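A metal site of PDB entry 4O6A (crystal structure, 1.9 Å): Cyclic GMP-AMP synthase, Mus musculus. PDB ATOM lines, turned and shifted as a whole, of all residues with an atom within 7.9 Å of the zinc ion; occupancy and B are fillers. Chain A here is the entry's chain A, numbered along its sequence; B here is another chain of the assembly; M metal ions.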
ATOM      1  N   LEU A 230     -21.574 -25.488 -24.051  1.00  0.00           N
ATOM      2  CA  LEU A 230     -20.416 -24.965 -24.767  1.00  0.00           C
ATOM      3  C   LEU A 230     -20.156 -23.474 -24.454  1.00  0.00           C
ATOM      4  O   LEU A 230     -18.998 -23.062 -24.341  1.00  0.00           O
ATOM      5  CB  LEU A 230     -20.562 -25.171 -26.270  1.00  0.00           C
ATOM      6  CG  LEU A 230     -19.842 -26.393 -26.887  1.00  0.00           C
ATOM      7  CD1 LEU A 230     -18.322 -26.287 -26.760  1.00  0.00           C
ATOM      8  CD2 LEU A 230     -20.313 -27.678 -26.277  1.00  0.00           C
ATOM      9  N   ASN A 231     -21.215 -22.688 -24.338  1.00  0.00           N
ATOM     10  CA  ASN A 231     -21.077 -21.245 -24.047  1.00  0.00           C
ATOM     11  C   ASN A 231     -20.955 -20.947 -22.559  1.00  0.00           C
ATOM     12  O   ASN A 231     -20.744 -19.802 -22.157  1.00  0.00           O
ATOM     13  CB  ASN A 231     -22.286 -20.457 -24.590  1.00  0.00           C
ATOM     14  CG  ASN A 231     -22.016 -18.934 -24.640  1.00  0.00           C
ATOM     15  OD1 ASN A 231     -20.968 -18.505 -25.124  1.00  0.00           O
ATOM     16  ND2 ASN A 231     -22.960 -18.135 -24.118  1.00  0.00           N
ATOM     17  N   ASN A 232     -21.117 -21.978 -21.731  1.00  0.00           N
ATOM     18  CA  ASN A 232     -21.114 -21.807 -20.279  1.00  0.00           C
ATOM     19  C   ASN A 232     -20.384 -22.967 -19.631  1.00  0.00           C
ATOM     20  O   ASN A 232     -20.969 -23.720 -18.854  1.00  0.00           O
ATOM     21  CB  ASN A 232     -22.549 -21.726 -19.731  1.00  0.00           C
ATOM     22  CG  ASN A 232     -23.291 -20.525 -20.240  1.00  0.00           C
ATOM     23  OD1 ASN A 232     -23.208 -19.429 -19.666  1.00  0.00           O
ATOM     24  ND2 ASN A 232     -24.009 -20.699 -21.350  1.00  0.00           N
ATOM     25  N   HIS A 233     -19.104 -23.110 -19.965  1.00  0.00           N
ATOM     26  CA  HIS A 233     -18.418 -24.390 -19.798  1.00  0.00           C
ATOM     27  C   HIS A 233     -17.451 -24.442 -18.631  1.00  0.00           C
ATOM     28  O   HIS A 233     -16.794 -25.462 -18.449  1.00  0.00           O
ATOM     29  CB  HIS A 233     -17.624 -24.701 -21.069  1.00  0.00           C
ATOM     30  CG  HIS A 233     -16.649 -23.626 -21.449  1.00  0.00           C
ATOM     31  ND1 HIS A 233     -16.771 -22.863 -22.583  1.00  0.00           N
ATOM     32  CD2 HIS A 233     -15.542 -23.176 -20.813  1.00  0.00           C
ATOM     33  CE1 HIS A 233     -15.784 -21.998 -22.645  1.00  0.00           C
ATOM     34  NE2 HIS A 233     -15.014 -22.172 -21.588  1.00  0.00           N
ATOM     35  N   GLY A 234     -17.341 -23.367 -17.884  1.00  0.00           N
ATOM     36  CA  GLY A 234     -16.325 -23.291 -16.852  1.00  0.00           C
ATOM     37  C   GLY A 234     -16.869 -23.601 -15.480  1.00  0.00           C
ATOM     38  O   GLY A 234     -18.054 -23.364 -15.209  1.00  0.00           O
ATOM     39  N   ILE A 235     -16.024 -24.124 -14.607  1.00  0.00           N
ATOM     40  CA  ILE A 235     -16.431 -24.206 -13.208  1.00  0.00           C
ATOM     41  C   ILE A 235     -16.533 -22.798 -12.628  1.00  0.00           C
ATOM     42  O   ILE A 235     -17.434 -22.517 -11.836  1.00  0.00           O
ATOM     43  CB  ILE A 235     -15.522 -25.111 -12.342  1.00  0.00           C
ATOM     44  CG1 ILE A 235     -16.116 -25.251 -10.938  1.00  0.00           C
ATOM     45  CG2 ILE A 235     -14.089 -24.598 -12.282  1.00  0.00           C
ATOM     46  CD1 ILE A 235     -15.641 -26.483 -10.204  1.00  0.00           C
ATOM     47  N   GLU A 236     -15.638 -21.910 -13.041  1.00  0.00           N
ATOM     48  CA  GLU A 236     -15.766 -20.498 -12.688  1.00  0.00           C
ATOM     49  C   GLU A 236     -16.649 -19.746 -13.683  1.00  0.00           C
ATOM     50  O   GLU A 236     -16.577 -19.972 -14.902  1.00  0.00           O
ATOM     51  CB  GLU A 236     -14.400 -19.807 -12.581  1.00  0.00           C
ATOM     52  CG  GLU A 236     -13.527 -20.338 -11.437  1.00  0.00           C
ATOM     53  CD  GLU A 236     -12.278 -19.496 -11.164  1.00  0.00           C
ATOM     54  OE1 GLU A 236     -12.015 -18.522 -11.899  1.00  0.00           O
ATOM     55  OE2 GLU A 236     -11.551 -19.804 -10.198  1.00  0.00           O
ATOM     56  N   THR A 238     -16.464 -16.812 -14.663  1.00  0.00           N
ATOM     57  CA  THR A 238     -15.716 -15.886 -15.504  1.00  0.00           C
ATOM     58  C   THR A 238     -14.871 -16.579 -16.591  1.00  0.00           C
ATOM     59  O   THR A 238     -14.111 -15.912 -17.300  1.00  0.00           O
ATOM     60  CB  THR A 238     -14.780 -15.006 -14.653  1.00  0.00           C
ATOM     61  OG1 THR A 238     -13.889 -15.852 -13.921  1.00  0.00           O
ATOM     62  CG2 THR A 238     -15.587 -14.157 -13.671  1.00  0.00           C
ATOM     63  N   CYS A 239     -14.977 -17.894 -16.710  1.00  0.00           N
ATOM     64  CA  CYS A 239     -14.141 -18.634 -17.675  1.00  0.00           C
ATOM     65  C   CYS A 239     -14.368 -18.105 -19.072  1.00  0.00           C
ATOM     66  O   CYS A 239     -15.518 -18.035 -19.533  1.00  0.00           O
ATOM     67  CB  CYS A 239     -14.452 -20.147 -17.630  1.00  0.00           C
ATOM     68  SG  CYS A 239     -13.297 -21.264 -18.560  1.00  0.00           S
ATOM     69  N   CYS A 240     -13.270 -17.725 -19.733  1.00  0.00           N
ATOM     70  CA  CYS A 240     -13.298 -17.180 -21.090  1.00  0.00           C
ATOM     71  C   CYS A 240     -14.048 -15.842 -21.227  1.00  0.00           C
ATOM     72  O   CYS A 240     -14.306 -15.409 -22.349  1.00  0.00           O
ATOM     73  CB  CYS A 240     -13.861 -18.195 -22.097  1.00  0.00           C
ATOM     74  SG  CYS A 240     -12.782 -19.672 -22.374  1.00  0.00           S
ATOM     75  N   GLU A 241     -14.399 -15.215 -20.111  1.00  0.00           N
ATOM     76  CA  GLU A 241     -15.002 -13.875 -20.133  1.00  0.00           C
ATOM     77  C   GLU A 241     -13.940 -12.792 -20.173  1.00  0.00           C
ATOM     78  O   GLU A 241     -12.756 -13.068 -19.947  1.00  0.00           O
ATOM     79  CB  GLU A 241     -15.914 -13.659 -18.926  1.00  0.00           C
ATOM     80  CG  GLU A 241     -17.171 -14.477 -18.941  1.00  0.00           C
ATOM     81  CD  GLU A 241     -18.132 -14.051 -17.884  1.00  0.00           C
ATOM     82  OE1 GLU A 241     -17.701 -13.363 -16.929  1.00  0.00           O
ATOM     83  OE2 GLU A 241     -19.318 -14.402 -18.005  1.00  0.00           O
ATOM     84  N   ALA A 245     -10.292 -15.778 -17.207  1.00  0.00           N
ATOM     85  CA  ALA A 245      -9.177 -16.407 -17.919  1.00  0.00           C
ATOM     86  C   ALA A 245      -9.650 -17.294 -19.054  1.00  0.00           C
ATOM     87  O   ALA A 245     -10.651 -18.002 -18.946  1.00  0.00           O
ATOM     88  CB  ALA A 245      -8.322 -17.228 -16.940  1.00  0.00           C
ATOM     89  N   LYS A 246      -8.919 -17.273 -20.170  1.00  0.00           N
ATOM     90  CA  LYS A 246      -9.176 -18.152 -21.303  1.00  0.00           C
ATOM     91  C   LYS A 246      -8.776 -19.573 -20.926  1.00  0.00           C
ATOM     92  O   LYS A 246      -7.708 -19.781 -20.332  1.00  0.00           O
ATOM     93  CB  LYS A 246      -8.322 -17.707 -22.495  1.00  0.00           C
ATOM     94  CG  LYS A 246      -8.617 -18.446 -23.787  1.00  0.00           C
ATOM     95  CD  LYS A 246      -9.889 -17.922 -24.436  1.00  0.00           C
ATOM     96  CE  LYS A 246     -10.193 -18.640 -25.730  1.00  0.00           C
ATOM     97  NZ  LYS A 246     -10.670 -20.032 -25.508  1.00  0.00           N
ATOM     98  N   CYS A 247      -9.621 -20.546 -21.245  1.00  0.00           N
ATOM     99  CA  CYS A 247      -9.267 -21.970 -21.125  1.00  0.00           C
ATOM    100  C   CYS A 247      -9.111 -22.556 -22.525  1.00  0.00           C
ATOM    101  O   CYS A 247      -9.358 -21.861 -23.520  1.00  0.00           O
ATOM    102  CB  CYS A 247     -10.345 -22.748 -20.337  1.00  0.00           C
ATOM    103  SG  CYS A 247     -11.867 -23.076 -21.268  1.00  0.00           S
ATOM    104  N   CYS A 248      -8.699 -23.818 -22.611  1.00  0.00           N
ATOM    105  CA  CYS A 248      -8.524 -24.440 -23.929  1.00  0.00           C
ATOM    106  C   CYS A 248      -9.522 -25.553 -24.233  1.00  0.00           C
ATOM    107  O   CYS A 248      -9.251 -26.416 -25.069  1.00  0.00           O
ATOM    108  CB  CYS A 248      -7.091 -24.976 -24.092  1.00  0.00           C
ATOM    109  SG  CYS A 248      -6.697 -26.464 -23.104  1.00  0.00           S
ATOM    110  N   ARG A 249     -10.676 -25.531 -23.582  1.00  0.00           N
ATOM    111  CA  ARG A 249     -11.659 -26.612 -23.759  1.00  0.00           C
ATOM    112  C   ARG A 249     -12.176 -26.688 -25.191  1.00  0.00           C
ATOM    113  O   ARG A 249     -12.216 -27.763 -25.790  1.00  0.00           O
ATOM    114  CB  ARG A 249     -12.836 -26.428 -22.805  1.00  0.00           C
ATOM    115  CG  ARG A 249     -12.521 -26.732 -21.337  1.00  0.00           C
ATOM    116  CD  ARG A 249     -13.823 -26.626 -20.559  1.00  0.00           C
ATOM    117  NE  ARG A 249     -13.721 -26.906 -19.124  1.00  0.00           N
ATOM    118  CZ  ARG A 249     -13.451 -26.005 -18.179  1.00  0.00           C
ATOM    119  NH1 ARG A 249     -13.180 -24.735 -18.515  1.00  0.00           N
ATOM    120  NH2 ARG A 249     -13.424 -26.364 -16.910  1.00  0.00           N
ATOM    121  N   LYS A 250     -12.554 -25.548 -25.749  1.00  0.00           N
ATOM    122  CA  LYS A 250     -13.096 -25.529 -27.110  1.00  0.00           C
ATOM    123  C   LYS A 250     -12.006 -25.868 -28.130  1.00  0.00           C
ATOM    124  O   LYS A 250     -12.262 -26.514 -29.141  1.00  0.00           O
ATOM    125  CB  LYS A 250     -13.711 -24.181 -27.418  1.00  0.00           C
ATOM    126  CG  LYS A 250     -14.968 -23.877 -26.599  1.00  0.00           C
ATOM    127  CD  LYS A 250     -15.528 -22.523 -27.013  1.00  0.00           C
ATOM    128  CE  LYS A 250     -16.942 -22.381 -26.485  1.00  0.00           C
ATOM    129  NZ  LYS A 250     -17.589 -21.141 -26.986  1.00  0.00           N
ATOM    130  N   GLU A 251     -10.800 -25.396 -27.864  1.00  0.00           N
ATOM    131  CA  GLU A 251      -9.674 -25.663 -28.757  1.00  0.00           C
ATOM    132  C   GLU A 251      -9.361 -27.165 -28.832  1.00  0.00           C
ATOM    133  O   GLU A 251      -9.050 -27.704 -29.895  1.00  0.00           O
ATOM    134  CB  GLU A 251      -8.454 -24.851 -28.335  1.00  0.00           C
ATOM    135  CG  GLU A 251      -8.600 -23.332 -28.558  1.00  0.00           C
ATOM    136  CD  GLU A 251      -9.561 -22.621 -27.582  1.00  0.00           C
ATOM    137  OE1 GLU A 251      -9.982 -21.484 -27.908  1.00  0.00           O
ATOM    138  OE2 GLU A 251      -9.904 -23.164 -26.509  1.00  0.00           O
ATOM    139  N   ASP A 292     -11.069 -25.354 -14.186  1.00  0.00           N
ATOM    140  CA  ASP A 292     -10.645 -24.577 -15.331  1.00  0.00           C
ATOM    141  C   ASP A 292      -9.133 -24.646 -15.435  1.00  0.00           C
ATOM    142  O   ASP A 292      -8.570 -24.545 -16.529  1.00  0.00           O
ATOM    143  CB  ASP A 292     -11.094 -23.126 -15.217  1.00  0.00           C
ATOM    144  CG  ASP A 292     -12.616 -22.982 -15.189  1.00  0.00           C
ATOM    145  OD1 ASP A 292     -13.304 -23.943 -15.573  1.00  0.00           O
ATOM    146  OD2 ASP A 292     -13.100 -21.899 -14.786  1.00  0.00           O
ATOM    147  N   TRP A 295      -7.554 -27.054 -17.769  1.00  0.00           N
ATOM    148  CA  TRP A 295      -7.703 -26.724 -19.189  1.00  0.00           C
ATOM    149  C   TRP A 295      -7.031 -25.390 -19.495  1.00  0.00           C
ATOM    150  O   TRP A 295      -7.569 -24.557 -20.245  1.00  0.00           O
ATOM    151  CB  TRP A 295      -9.188 -26.725 -19.577  1.00  0.00           C
ATOM    152  CG  TRP A 295      -9.793 -28.067 -19.329  1.00  0.00           C
ATOM    153  CD1 TRP A 295     -10.408 -28.491 -18.189  1.00  0.00           C
ATOM    154  CD2 TRP A 295      -9.788 -29.184 -20.226  1.00  0.00           C
ATOM    155  NE1 TRP A 295     -10.799 -29.811 -18.328  1.00  0.00           N
ATOM    156  CE2 TRP A 295     -10.433 -30.249 -19.568  1.00  0.00           C
ATOM    157  CE3 TRP A 295      -9.314 -29.379 -21.526  1.00  0.00           C
ATOM    158  CZ2 TRP A 295     -10.610 -31.503 -20.168  1.00  0.00           C
ATOM    159  CZ3 TRP A 295      -9.490 -30.623 -22.125  1.00  0.00           C
ATOM    160  CH2 TRP A 295     -10.133 -31.660 -21.443  1.00  0.00           C
ATOM    161  P    DA B  11     -15.743 -17.943 -27.642  1.00  0.00           P
ATOM    162  OP1  DA B  11     -16.073 -19.279 -28.192  1.00  0.00           O
ATOM    163  OP2  DA B  11     -14.931 -17.818 -26.399  1.00  0.00           O
ATOM    164  O5'  DA B  11     -15.003 -17.101 -28.761  1.00  0.00           O
ATOM    165  C5'  DA B  11     -15.568 -17.144 -30.071  1.00  0.00           C
ATOM    166  C4'  DA B  11     -14.845 -16.146 -30.950  1.00  0.00           C
ATOM    167  O4'  DA B  11     -15.156 -14.831 -30.451  1.00  0.00           O
ATOM    168  C3'  DA B  11     -13.318 -16.231 -30.962  1.00  0.00           C
ATOM    169  O3'  DA B  11     -12.893 -15.896 -32.252  1.00  0.00           O
ATOM    170  C2'  DA B  11     -12.900 -15.133 -29.989  1.00  0.00           C
ATOM    171  C1'  DA B  11     -13.963 -14.115 -30.393  1.00  0.00           C
ATOM    172  N9   DA B  11     -14.105 -12.955 -29.529  1.00  0.00           N
ATOM    173  C8   DA B  11     -13.886 -12.810 -28.183  1.00  0.00           C
ATOM    174  N7   DA B  11     -14.081 -11.571 -27.759  1.00  0.00           N
ATOM    175  C5   DA B  11     -14.456 -10.885 -28.916  1.00  0.00           C
ATOM    176  C6   DA B  11     -14.815  -9.553 -29.162  1.00  0.00           C
ATOM    177  N6   DA B  11     -14.858  -8.609 -28.215  1.00  0.00           N
ATOM    178  N1   DA B  11     -15.134  -9.231 -30.435  1.00  0.00           N
ATOM    179  C2   DA B  11     -15.088 -10.175 -31.392  1.00  0.00           C
ATOM    180  N3   DA B  11     -14.778 -11.457 -31.283  1.00  0.00           N
ATOM    181  C4   DA B  11     -14.468 -11.739 -30.011  1.00  0.00           C
HETATM  182 ZN    ZN M   1     -13.344 -21.284 -20.835  1.00  0.00          ZN
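The zinc ion is bound by a ring nitrogen (NE2) of His 233 (2.0 Å), the side-chain sulfur (SG) of Cys 239 (2.3 Å), the side-chain sulfur (SG) of Cys 240 (2.3 Å) and the side-chain sulfur (SG) of Cys 247 (2.4 Å).
The zinc ion has four donor atoms within binding distance.
Within 4 Å of the zinc ion: His 233, Cys 239, Cys 240 and Cys 247.
NE of Arg 249 sits close to O of His 233, 3.5 Å away.
The backbone carbonyl oxygen of Leu 230 lies within hydrogen-bond range of a ring nitrogen (ND1) of His 233 (2.8 Å).
SG of Cys 239 sits close to NH1 of Arg 249 (3.5 Å).
The backbone NH (N) of Cys 240 lies within hydrogen-bond range of the backbone carbonyl oxygen (O) of Ala 245.
SG of Cys 240 lies close to NZ of Lys 246, 3.8 Å away.
The side-chain sulfur of Cys 247 sits close to the guanidinium group of Arg 249, 3.5 Å away.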
